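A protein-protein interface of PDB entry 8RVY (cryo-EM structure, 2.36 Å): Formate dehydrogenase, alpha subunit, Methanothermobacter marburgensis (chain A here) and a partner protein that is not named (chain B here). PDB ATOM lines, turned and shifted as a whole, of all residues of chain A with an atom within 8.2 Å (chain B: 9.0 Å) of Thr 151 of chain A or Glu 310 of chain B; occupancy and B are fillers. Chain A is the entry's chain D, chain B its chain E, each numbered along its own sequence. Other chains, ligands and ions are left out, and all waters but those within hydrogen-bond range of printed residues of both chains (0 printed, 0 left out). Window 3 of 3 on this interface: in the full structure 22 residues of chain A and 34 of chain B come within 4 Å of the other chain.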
ATOM      1  N   SER A  10      33.941  16.002  24.053  1.00  0.00           N
ATOM      2  CA  SER A  10      33.264  17.280  24.211  1.00  0.00           C
ATOM      3  C   SER A  10      31.889  17.170  24.858  1.00  0.00           C
ATOM      4  O   SER A  10      31.335  18.196  25.260  1.00  0.00           O
ATOM      5  CB  SER A  10      33.144  17.969  22.855  1.00  0.00           C
ATOM      6  OG  SER A  10      34.421  18.320  22.362  1.00  0.00           O
ATOM      7  N   CYS A  11      31.321  15.974  24.967  1.00  0.00           N
ATOM      8  CA  CYS A  11      30.155  15.773  25.816  1.00  0.00           C
ATOM      9  C   CYS A  11      30.060  14.288  26.134  1.00  0.00           C
ATOM     10  O   CYS A  11      30.914  13.491  25.739  1.00  0.00           O
ATOM     11  CB  CYS A  11      28.865  16.285  25.169  1.00  0.00           C
ATOM     12  SG  CYS A  11      28.145  15.214  23.926  1.00  0.00           S
ATOM     13  N   CYS A  43      29.067  16.600  15.718  1.00  0.00           N
ATOM     14  CA  CYS A  43      28.758  18.017  15.750  1.00  0.00           C
ATOM     15  C   CYS A  43      30.051  18.814  15.611  1.00  0.00           C
ATOM     16  O   CYS A  43      31.143  18.257  15.498  1.00  0.00           O
ATOM     17  CB  CYS A  43      28.017  18.368  17.036  1.00  0.00           C
ATOM     18  SG  CYS A  43      29.030  18.283  18.527  1.00  0.00           S
ATOM     19  N   ALA A  45      31.664  20.421  17.778  1.00  0.00           N
ATOM     20  CA  ALA A  45      32.574  20.155  18.887  1.00  0.00           C
ATOM     21  C   ALA A  45      33.398  18.899  18.638  1.00  0.00           C
ATOM     22  O   ALA A  45      34.567  18.827  19.031  1.00  0.00           O
ATOM     23  CB  ALA A  45      31.793  20.029  20.190  1.00  0.00           C
ATOM     24  N   GLY A 147      14.951  19.316  29.595  1.00  0.00           N
ATOM     25  CA  GLY A 147      16.131  19.990  29.097  1.00  0.00           C
ATOM     26  C   GLY A 147      16.159  20.019  27.583  1.00  0.00           C
ATOM     27  O   GLY A 147      15.211  19.627  26.895  1.00  0.00           O
ATOM     28  N   ASP A 148      17.281  20.503  27.058  1.00  0.00           N
ATOM     29  CA  ASP A 148      17.504  20.588  25.616  1.00  0.00           C
ATOM     30  C   ASP A 148      18.456  19.464  25.225  1.00  0.00           C
ATOM     31  O   ASP A 148      19.668  19.652  25.129  1.00  0.00           O
ATOM     32  CB  ASP A 148      18.050  21.957  25.229  1.00  0.00           C
ATOM     33  CG  ASP A 148      17.901  22.247  23.750  1.00  0.00           C
ATOM     34  OD1 ASP A 148      17.125  21.539  23.076  1.00  0.00           O
ATOM     35  OD2 ASP A 148      18.562  23.183  23.257  1.00  0.00           O
ATOM     36  N   ALA A 149      17.890  18.281  24.983  1.00  0.00           N
ATOM     37  CA  ALA A 149      18.713  17.114  24.687  1.00  0.00           C
ATOM     38  C   ALA A 149      19.437  17.261  23.357  1.00  0.00           C
ATOM     39  O   ALA A 149      20.573  16.798  23.211  1.00  0.00           O
ATOM     40  CB  ALA A 149      17.849  15.856  24.690  1.00  0.00           C
ATOM     41  N   ILE A 150      18.797  17.895  22.371  1.00  0.00           N
ATOM     42  CA  ILE A 150      19.428  18.054  21.065  1.00  0.00           C
ATOM     43  C   ILE A 150      20.685  18.905  21.178  1.00  0.00           C
ATOM     44  O   ILE A 150      21.713  18.601  20.565  1.00  0.00           O
ATOM     45  CB  ILE A 150      18.434  18.651  20.053  1.00  0.00           C
ATOM     46  CG1 ILE A 150      17.324  17.649  19.739  1.00  0.00           C
ATOM     47  CG2 ILE A 150      19.159  19.050  18.780  1.00  0.00           C
ATOM     48  CD1 ILE A 150      16.157  18.241  18.990  1.00  0.00           C
ATOM     49  N   THR A 151      20.623  19.991  21.945  1.00  0.00           N
ATOM     50  CA  THR A 151      21.782  20.871  22.048  1.00  0.00           C
ATOM     51  C   THR A 151      22.859  20.282  22.948  1.00  0.00           C
ATOM     52  O   THR A 151      24.052  20.448  22.678  1.00  0.00           O
ATOM     53  CB  THR A 151      21.358  22.245  22.564  1.00  0.00           C
ATOM     54  OG1 THR A 151      20.537  22.893  21.586  1.00  0.00           O
ATOM     55  CG2 THR A 151      22.580  23.107  22.852  1.00  0.00           C
ATOM     56  N   CYS A 152      22.466  19.608  24.030  1.00  0.00           N
ATOM     57  CA  CYS A 152      23.451  19.051  24.952  1.00  0.00           C
ATOM     58  C   CYS A 152      24.284  17.972  24.275  1.00  0.00           C
ATOM     59  O   CYS A 152      25.517  18.017  24.296  1.00  0.00           O
ATOM     60  CB  CYS A 152      22.753  18.496  26.190  1.00  0.00           C
ATOM     61  SG  CYS A 152      22.157  19.754  27.330  1.00  0.00           S
ATOM     62  N   ALA A 153      23.623  16.994  23.664  1.00  0.00           N
ATOM     63  CA  ALA A 153      24.288  15.941  22.899  1.00  0.00           C
ATOM     64  C   ALA A 153      23.552  15.784  21.574  1.00  0.00           C
ATOM     65  O   ALA A 153      22.541  15.066  21.506  1.00  0.00           O
ATOM     66  CB  ALA A 153      24.316  14.628  23.671  1.00  0.00           C
ATOM     67  N   PRO A 154      24.012  16.443  20.510  1.00  0.00           N
ATOM     68  CA  PRO A 154      23.294  16.350  19.228  1.00  0.00           C
ATOM     69  C   PRO A 154      23.084  14.930  18.730  1.00  0.00           C
ATOM     70  O   PRO A 154      22.046  14.645  18.117  1.00  0.00           O
ATOM     71  CB  PRO A 154      24.192  17.150  18.277  1.00  0.00           C
ATOM     72  CG  PRO A 154      24.908  18.108  19.138  1.00  0.00           C
ATOM     73  CD  PRO A 154      25.055  17.482  20.488  1.00  0.00           C
ATOM     74  N   LEU A 155      24.032  14.027  18.970  1.00  0.00           N
ATOM     75  CA  LEU A 155      23.947  12.692  18.396  1.00  0.00           C
ATOM     76  C   LEU A 155      22.986  11.775  19.143  1.00  0.00           C
ATOM     77  O   LEU A 155      22.699  10.681  18.650  1.00  0.00           O
ATOM     78  CB  LEU A 155      25.342  12.064  18.335  1.00  0.00           C
ATOM     79  CG  LEU A 155      26.096  12.288  17.018  1.00  0.00           C
ATOM     80  CD1 LEU A 155      25.331  11.704  15.844  1.00  0.00           C
ATOM     81  CD2 LEU A 155      26.374  13.765  16.779  1.00  0.00           C
ATOM     82  N   ILE A 156      22.479  12.187  20.302  1.00  0.00           N
ATOM     83  CA  ILE A 156      21.336  11.505  20.901  1.00  0.00           C
ATOM     84  C   ILE A 156      20.023  12.151  20.458  1.00  0.00           C
ATOM     85  O   ILE A 156      18.997  11.468  20.349  1.00  0.00           O
ATOM     86  CB  ILE A 156      21.464  11.488  22.434  1.00  0.00           C
ATOM     87  CG1 ILE A 156      22.588  10.544  22.857  1.00  0.00           C
ATOM     88  CG2 ILE A 156      20.163  11.048  23.077  1.00  0.00           C
ATOM     89  CD1 ILE A 156      23.416  11.055  24.005  1.00  0.00           C
ATOM     90  N   GLY A 157      20.032  13.457  20.186  1.00  0.00           N
ATOM     91  CA  GLY A 157      18.885  14.067  19.540  1.00  0.00           C
ATOM     92  C   GLY A 157      18.611  13.460  18.182  1.00  0.00           C
ATOM     93  O   GLY A 157      17.461  13.399  17.741  1.00  0.00           O
ATOM     94  N   ILE A 160      16.492  10.634  18.959  1.00  0.00           N
ATOM     95  CA  ILE A 160      15.145  11.125  19.252  1.00  0.00           C
ATOM     96  C   ILE A 160      14.382  11.380  17.956  1.00  0.00           C
ATOM     97  O   ILE A 160      13.184  11.085  17.850  1.00  0.00           O
ATOM     98  CB  ILE A 160      15.202  12.390  20.129  1.00  0.00           C
ATOM     99  CG1 ILE A 160      15.922  12.104  21.446  1.00  0.00           C
ATOM    100  CG2 ILE A 160      13.795  12.899  20.401  1.00  0.00           C
ATOM    101  CD1 ILE A 160      16.271  13.352  22.229  1.00  0.00           C
ATOM    102  N   ARG A 176      12.322  27.184  28.919  1.00  0.00           N
ATOM    103  CA  ARG A 176      12.437  28.032  27.744  1.00  0.00           C
ATOM    104  C   ARG A 176      11.513  27.530  26.642  1.00  0.00           C
ATOM    105  O   ARG A 176      11.229  26.333  26.543  1.00  0.00           O
ATOM    106  CB  ARG A 176      13.884  28.074  27.249  1.00  0.00           C
ATOM    107  CG  ARG A 176      14.816  28.837  28.181  1.00  0.00           C
ATOM    108  CD  ARG A 176      16.260  28.352  28.107  1.00  0.00           C
ATOM    109  NE  ARG A 176      16.381  26.909  28.293  1.00  0.00           N
ATOM    110  CZ  ARG A 176      17.088  26.096  27.517  1.00  0.00           C
ATOM    111  NH1 ARG A 176      17.775  26.545  26.480  1.00  0.00           N
ATOM    112  NH2 ARG A 176      17.107  24.795  27.791  1.00  0.00           N
ATOM    113  N   GLU A 178      11.859  28.591  23.184  1.00  0.00           N
ATOM    114  CA  GLU A 178      12.504  28.578  21.876  1.00  0.00           C
ATOM    115  C   GLU A 178      13.853  27.869  22.019  1.00  0.00           C
ATOM    116  O   GLU A 178      14.900  28.477  22.238  1.00  0.00           O
ATOM    117  CB  GLU A 178      12.671  29.994  21.320  1.00  0.00           C
ATOM    118  N   THR A 179      13.820  26.548  21.892  1.00  0.00           N
ATOM    119  CA  THR A 179      15.001  25.704  21.912  1.00  0.00           C
ATOM    120  C   THR A 179      14.822  24.614  20.869  1.00  0.00           C
ATOM    121  O   THR A 179      13.701  24.317  20.447  1.00  0.00           O
ATOM    122  CB  THR A 179      15.237  25.088  23.299  1.00  0.00           C
ATOM    123  OG1 THR A 179      14.392  23.945  23.472  1.00  0.00           O
ATOM    124  CG2 THR A 179      14.943  26.094  24.389  1.00  0.00           C
ATOM    125  N   ARG A 180      15.937  24.017  20.447  1.00  0.00           N
ATOM    126  CA  ARG A 180      15.867  23.046  19.360  1.00  0.00           C
ATOM    127  C   ARG A 180      14.919  21.908  19.706  1.00  0.00           C
ATOM    128  O   ARG A 180      14.075  21.523  18.888  1.00  0.00           O
ATOM    129  CB  ARG A 180      17.261  22.515  19.039  1.00  0.00           C
ATOM    130  CG  ARG A 180      18.181  23.580  18.486  1.00  0.00           C
ATOM    131  CD  ARG A 180      19.511  23.023  18.029  1.00  0.00           C
ATOM    132  NE  ARG A 180      19.926  23.658  16.784  1.00  0.00           N
ATOM    133  CZ  ARG A 180      20.948  24.494  16.656  1.00  0.00           C
ATOM    134  NH1 ARG A 180      21.733  24.794  17.677  1.00  0.00           N
ATOM    135  NH2 ARG A 180      21.187  25.047  15.472  1.00  0.00           N
ATOM    136  N   MET A 181      15.033  21.364  20.918  1.00  0.00           N
ATOM    137  CA  MET A 181      14.113  20.317  21.340  1.00  0.00           C
ATOM    138  C   MET A 181      12.687  20.842  21.425  1.00  0.00           C
ATOM    139  O   MET A 181      11.749  20.178  20.974  1.00  0.00           O
ATOM    140  CB  MET A 181      14.559  19.742  22.682  1.00  0.00           C
ATOM    141  CG  MET A 181      13.819  18.485  23.081  1.00  0.00           C
ATOM    142  SD  MET A 181      14.322  17.060  22.105  1.00  0.00           S
ATOM    143  CE  MET A 181      12.725  16.392  21.665  1.00  0.00           C
ATOM    144  N   ALA A 182      12.504  22.038  21.982  1.00  0.00           N
ATOM    145  CA  ALA A 182      11.172  22.629  22.043  1.00  0.00           C
ATOM    146  C   ALA A 182      10.604  22.828  20.646  1.00  0.00           C
ATOM    147  O   ALA A 182       9.422  22.564  20.396  1.00  0.00           O
ATOM    148  CB  ALA A 182      11.226  23.958  22.794  1.00  0.00           C
ATOM    149  N   VAL A 183      11.438  23.300  19.719  1.00  0.00           N
ATOM    150  CA  VAL A 183      10.988  23.541  18.353  1.00  0.00           C
ATOM    151  C   VAL A 183      10.572  22.237  17.684  1.00  0.00           C
ATOM    152  O   VAL A 183       9.533  22.170  17.017  1.00  0.00           O
ATOM    153  CB  VAL A 183      12.098  24.257  17.556  1.00  0.00           C
ATOM    154  CG1 VAL A 183      11.939  24.018  16.066  1.00  0.00           C
ATOM    155  CG2 VAL A 183      12.094  25.742  17.861  1.00  0.00           C
ATOM    156  N   ASN A 184      11.372  21.181  17.850  1.00  0.00           N
ATOM    157  CA  ASN A 184      11.228  19.983  17.032  1.00  0.00           C
ATOM    158  C   ASN A 184      10.365  18.899  17.661  1.00  0.00           C
ATOM    159  O   ASN A 184       9.883  18.023  16.937  1.00  0.00           O
ATOM    160  CB  ASN A 184      12.606  19.395  16.723  1.00  0.00           C
ATOM    161  CG  ASN A 184      13.410  20.265  15.785  1.00  0.00           C
ATOM    162  OD1 ASN A 184      13.118  20.350  14.596  1.00  0.00           O
ATOM    163  ND2 ASN A 184      14.430  20.921  16.317  1.00  0.00           N
ATOM    164  N   THR A 213      18.514  16.100  30.922  1.00  0.00           N
ATOM    165  CA  THR A 213      19.791  16.785  30.807  1.00  0.00           C
ATOM    166  C   THR A 213      20.107  17.532  32.089  1.00  0.00           C
ATOM    167  O   THR A 213      19.286  17.604  33.007  1.00  0.00           O
ATOM    168  CB  THR A 213      19.769  17.757  29.628  1.00  0.00           C
ATOM    169  OG1 THR A 213      19.166  18.985  30.043  1.00  0.00           O
ATOM    170  CG2 THR A 213      18.988  17.186  28.462  1.00  0.00           C
ATOM    171  N   GLU A 215      20.281  20.690  32.429  1.00  0.00           N
ATOM    172  CA  GLU A 215      19.843  22.080  32.326  1.00  0.00           C
ATOM    173  C   GLU A 215      19.097  22.516  33.580  1.00  0.00           C
ATOM    174  O   GLU A 215      19.294  23.632  34.075  1.00  0.00           O
ATOM    175  CB  GLU A 215      18.961  22.263  31.087  1.00  0.00           C
ATOM    176  CG  GLU A 215      19.666  22.080  29.741  1.00  0.00           C
ATOM    177  CD  GLU A 215      21.142  22.420  29.784  1.00  0.00           C
ATOM    178  OE1 GLU A 215      21.963  21.490  29.932  1.00  0.00           O
ATOM    179  OE2 GLU A 215      21.482  23.617  29.672  1.00  0.00           O
ATOM    180  N   ILE A 237      21.908  12.746  30.643  1.00  0.00           N
ATOM    181  CA  ILE A 237      22.934  13.337  29.797  1.00  0.00           C
ATOM    182  C   ILE A 237      23.925  14.063  30.694  1.00  0.00           C
ATOM    183  O   ILE A 237      23.758  15.245  31.002  1.00  0.00           O
ATOM    184  CB  ILE A 237      22.318  14.267  28.738  1.00  0.00           C
ATOM    185  CG1 ILE A 237      21.564  13.435  27.705  1.00  0.00           C
ATOM    186  CG2 ILE A 237      23.394  15.080  28.051  1.00  0.00           C
ATOM    187  CD1 ILE A 237      20.407  14.145  27.077  1.00  0.00           C
ATOM    188  N   LYS B 278      14.220  22.101   9.057  1.00  0.00           N
ATOM    189  CA  LYS B 278      13.992  22.473  10.448  1.00  0.00           C
ATOM    190  C   LYS B 278      14.968  21.788  11.395  1.00  0.00           C
ATOM    191  O   LYS B 278      15.209  22.297  12.494  1.00  0.00           O
ATOM    192  CB  LYS B 278      12.563  22.126  10.856  1.00  0.00           C
ATOM    193  CG  LYS B 278      11.532  23.136  10.406  1.00  0.00           C
ATOM    194  CD  LYS B 278      10.123  22.697  10.771  1.00  0.00           C
ATOM    195  CE  LYS B 278       9.221  22.648   9.546  1.00  0.00           C
ATOM    196  NZ  LYS B 278       9.127  23.965   8.857  1.00  0.00           N
ATOM    197  N   CYS B 280      18.277  21.106  10.940  1.00  0.00           N
ATOM    198  CA  CYS B 280      19.695  21.421  10.824  1.00  0.00           C
ATOM    199  C   CYS B 280      20.213  22.118  12.075  1.00  0.00           C
ATOM    200  O   CYS B 280      19.590  23.052  12.584  1.00  0.00           O
ATOM    201  CB  CYS B 280      19.926  22.296   9.594  1.00  0.00           C
ATOM    202  SG  CYS B 280      21.642  22.749   9.299  1.00  0.00           S
ATOM    203  N   ILE B 281      21.367  21.663  12.562  1.00  0.00           N
ATOM    204  CA  ILE B 281      21.993  22.225  13.753  1.00  0.00           C
ATOM    205  C   ILE B 281      23.189  23.106  13.410  1.00  0.00           C
ATOM    206  O   ILE B 281      23.918  23.527  14.311  1.00  0.00           O
ATOM    207  CB  ILE B 281      22.403  21.123  14.743  1.00  0.00           C
ATOM    208  CG1 ILE B 281      23.292  20.081  14.060  1.00  0.00           C
ATOM    209  CG2 ILE B 281      21.179  20.466  15.342  1.00  0.00           C
ATOM    210  CD1 ILE B 281      24.332  19.485  14.968  1.00  0.00           C
ATOM    211  N   ASN B 282      23.413  23.392  12.129  1.00  0.00           N
ATOM    212  CA  ASN B 282      24.419  24.368  11.722  1.00  0.00           C
ATOM    213  C   ASN B 282      25.820  23.930  12.141  1.00  0.00           C
ATOM    214  O   ASN B 282      26.671  24.750  12.484  1.00  0.00           O
ATOM    215  CB  ASN B 282      24.083  25.744  12.299  1.00  0.00           C
ATOM    216  CG  ASN B 282      24.622  26.881  11.462  1.00  0.00           C
ATOM    217  OD1 ASN B 282      24.847  26.735  10.263  1.00  0.00           O
ATOM    218  ND2 ASN B 282      24.821  28.031  12.091  1.00  0.00           N
ATOM    219  N   CYS B 283      26.064  22.621  12.112  1.00  0.00           N
ATOM    220  CA  CYS B 283      27.343  22.078  12.549  1.00  0.00           C
ATOM    221  C   CYS B 283      28.414  22.128  11.470  1.00  0.00           C
ATOM    222  O   CYS B 283      29.599  22.031  11.797  1.00  0.00           O
ATOM    223  CB  CYS B 283      27.161  20.635  13.018  1.00  0.00           C
ATOM    224  SG  CYS B 283      26.781  19.462  11.703  1.00  0.00           S
ATOM    225  N   LEU B 306      26.000  33.725   8.407  1.00  0.00           N
ATOM    226  CA  LEU B 306      25.957  32.751   9.486  1.00  0.00           C
ATOM    227  C   LEU B 306      24.740  32.961  10.376  1.00  0.00           C
ATOM    228  O   LEU B 306      24.367  34.092  10.696  1.00  0.00           O
ATOM    229  CB  LEU B 306      27.238  32.850  10.313  1.00  0.00           C
ATOM    230  CG  LEU B 306      27.481  31.788  11.383  1.00  0.00           C
ATOM    231  CD1 LEU B 306      27.486  30.392  10.788  1.00  0.00           C
ATOM    232  CD2 LEU B 306      28.791  32.075  12.082  1.00  0.00           C
ATOM    233  N   GLU B 307      24.127  31.854  10.783  1.00  0.00           N
ATOM    234  CA  GLU B 307      23.024  31.886  11.735  1.00  0.00           C
ATOM    235  C   GLU B 307      23.568  32.131  13.138  1.00  0.00           C
ATOM    236  O   GLU B 307      24.309  31.301  13.675  1.00  0.00           O
ATOM    237  CB  GLU B 307      22.225  30.586  11.653  1.00  0.00           C
ATOM    238  CG  GLU B 307      21.209  30.385  12.764  1.00  0.00           C
ATOM    239  CD  GLU B 307      20.161  31.473  12.801  1.00  0.00           C
ATOM    240  OE1 GLU B 307      19.126  31.329  12.117  1.00  0.00           O
ATOM    241  OE2 GLU B 307      20.374  32.476  13.510  1.00  0.00           O
ATOM    242  N   SER B 308      23.218  33.279  13.720  1.00  0.00           N
ATOM    243  CA  SER B 308      23.725  33.632  15.042  1.00  0.00           C
ATOM    244  C   SER B 308      23.068  32.805  16.141  1.00  0.00           C
ATOM    245  O   SER B 308      23.755  32.291  17.029  1.00  0.00           O
ATOM    246  CB  SER B 308      23.519  35.126  15.295  1.00  0.00           C
ATOM    247  OG  SER B 308      23.970  35.491  16.585  1.00  0.00           O
ATOM    248  N   ASP B 309      21.748  32.660  16.092  1.00  0.00           N
ATOM    249  CA  ASP B 309      21.033  31.986  17.163  1.00  0.00           C
ATOM    250  C   ASP B 309      21.251  30.477  17.135  1.00  0.00           C
ATOM    251  O   ASP B 309      21.716  29.903  16.148  1.00  0.00           O
ATOM    252  CB  ASP B 309      19.539  32.292  17.048  1.00  0.00           C
ATOM    253  CG  ASP B 309      19.264  33.714  16.606  1.00  0.00           C
ATOM    254  OD1 ASP B 309      19.522  34.032  15.426  1.00  0.00           O
ATOM    255  OD2 ASP B 309      18.790  34.516  17.437  1.00  0.00           O
ATOM    256  N   GLU B 310      20.907  29.834  18.249  1.00  0.00           N
ATOM    257  CA  GLU B 310      20.960  28.377  18.346  1.00  0.00           C
ATOM    258  C   GLU B 310      19.648  27.796  17.820  1.00  0.00           C
ATOM    259  O   GLU B 310      18.845  27.205  18.543  1.00  0.00           O
ATOM    260  CB  GLU B 310      21.239  27.947  19.780  1.00  0.00           C
ATOM    261  CG  GLU B 310      22.718  27.852  20.123  1.00  0.00           C
ATOM    262  CD  GLU B 310      23.430  26.749  19.360  1.00  0.00           C
ATOM    263  OE1 GLU B 310      23.451  25.601  19.850  1.00  0.00           O
ATOM    264  OE2 GLU B 310      23.967  27.029  18.267  1.00  0.00           O
ATOM    265  N   LYS B 311      19.444  27.987  16.519  1.00  0.00           N
ATOM    266  CA  LYS B 311      18.261  27.490  15.833  1.00  0.00           C
ATOM    267  C   LYS B 311      18.661  27.081  14.423  1.00  0.00           C
ATOM    268  O   LYS B 311      19.793  27.301  13.990  1.00  0.00           O
ATOM    269  CB  LYS B 311      17.149  28.542  15.808  1.00  0.00           C
ATOM    270  CG  LYS B 311      17.427  29.716  14.892  1.00  0.00           C
ATOM    271  CD  LYS B 311      16.546  30.900  15.227  1.00  0.00           C
ATOM    272  CE  LYS B 311      16.410  31.842  14.045  1.00  0.00           C
ATOM    273  NZ  LYS B 311      16.515  33.268  14.448  1.00  0.00           N
ATOM    274  N   ALA B 312      17.718  26.478  13.709  1.00  0.00           N
ATOM    275  CA  ALA B 312      18.008  25.991  12.370  1.00  0.00           C
ATOM    276  C   ALA B 312      18.336  27.164  11.449  1.00  0.00           C
ATOM    277  O   ALA B 312      17.662  28.198  11.500  1.00  0.00           O
ATOM    278  CB  ALA B 312      16.821  25.206  11.813  1.00  0.00           C
ATOM    279  N   PRO B 313      19.350  27.045  10.596  1.00  0.00           N
ATOM    280  CA  PRO B 313      19.634  28.123   9.646  1.00  0.00           C
ATOM    281  C   PRO B 313      18.531  28.250   8.610  1.00  0.00           C
ATOM    282  O   PRO B 313      17.765  27.320   8.354  1.00  0.00           O
ATOM    283  CB  PRO B 313      20.954  27.701   8.990  1.00  0.00           C
ATOM    284  CG  PRO B 313      21.441  26.533   9.748  1.00  0.00           C
ATOM    285  CD  PRO B 313      20.273  25.914  10.420  1.00  0.00           C
ATOM    286  N   MET B 342      21.965  14.980  11.513  1.00  0.00           N
ATOM    287  CA  MET B 342      20.515  15.073  11.528  1.00  0.00           C
ATOM    288  C   MET B 342      19.848  14.199  10.477  1.00  0.00           C
ATOM    289  O   MET B 342      18.618  14.208  10.379  1.00  0.00           O
ATOM    290  CB  MET B 342      20.093  16.534  11.333  1.00  0.00           C
ATOM    291  CG  MET B 342      20.121  17.380  12.602  1.00  0.00           C
ATOM    292  SD  MET B 342      19.382  16.616  14.060  1.00  0.00           S
ATOM    293  CE  MET B 342      20.794  16.514  15.151  1.00  0.00           C
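CG2 of Thr 151 of chain A touches OE1 of Glu 310 of chain B (3.999 Å).
O of Pro 154 of chain A touches CE of Met 342 of chain B, at 3.7 Å.
O of Cys 280 of chain B touches NH2 of Arg 180 of chain A, 3.9 Å away.
Asn 184 of chain A touches Lys 278 of chain B (OD1 to O, 3.5 Å).
NH1 of Arg 180 of chain A lies within salt-bridge range of OE1 of Glu 310 of chain B.
NH2 of Arg 180 of chain A is in hydrogen-bond range of O of Ile 281 of chain B (3.3 Å).
NH2 of Arg 180 of chain A sits at hydrogen-bond distance from O of Lys 311 of chain B (3.0 Å).
Printed residues of chain B within 4 Å of Thr 151 of chain A: Glu 310 (3.999 Å).
Printed residues of chain A within 4 Å of Glu 310 of chain B: Thr 151 and Arg 180.
No residue of chain B comes within 4 Å of Cys 152 of chain A.
Of the printed residues of chain A, Lys 278 of chain B touches Asn 184.
Of the printed residues of chain B, Asn 184 of chain A touches Lys 278 (3.5 Å).
Of the printed residues of chain B, Arg 180 of chain A touches Cys 280, Ile 281, Glu 310 and Lys 311.
The nearest printed residue of chain A that does not touch Glu 310 of chain B is Thr 179 of chain A (5.3 Å).
OD1 of Asp 309 of chain B is in salt-bridge range of NZ of Lys 311 of chain B (3.3 Å).
The side-chain sulfur of Cys 280 of chain B sits close to the backbone NH of Asn 282 of chain B (3.4 Å).
ND2 of Asn 184 of chain A is in hydrogen-bond range of O of Arg 180 of chain A.
The side-chain hydroxyl (OG1) of Thr 151 of chain A lies within hydrogen-bond range of the side-chain carboxylate (OD2) of Asp 148 of chain A (2.6 Å).
Along chain A the printed residues that touch a printed residue of chain B span positions 151 to 184.
Printed residues of chain B that touch a printed residue of chain A: Lys 278, Cys 280, Ile 281, Glu 310, Lys 311 and Met 342.
Among the printed residues, Asp or Glu carboxylates within 4 Å of a Lys or Arg side-chain nitrogen of the other chain: Arg 180 of chain A with Glu 310 of chain B (2.9 Å).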
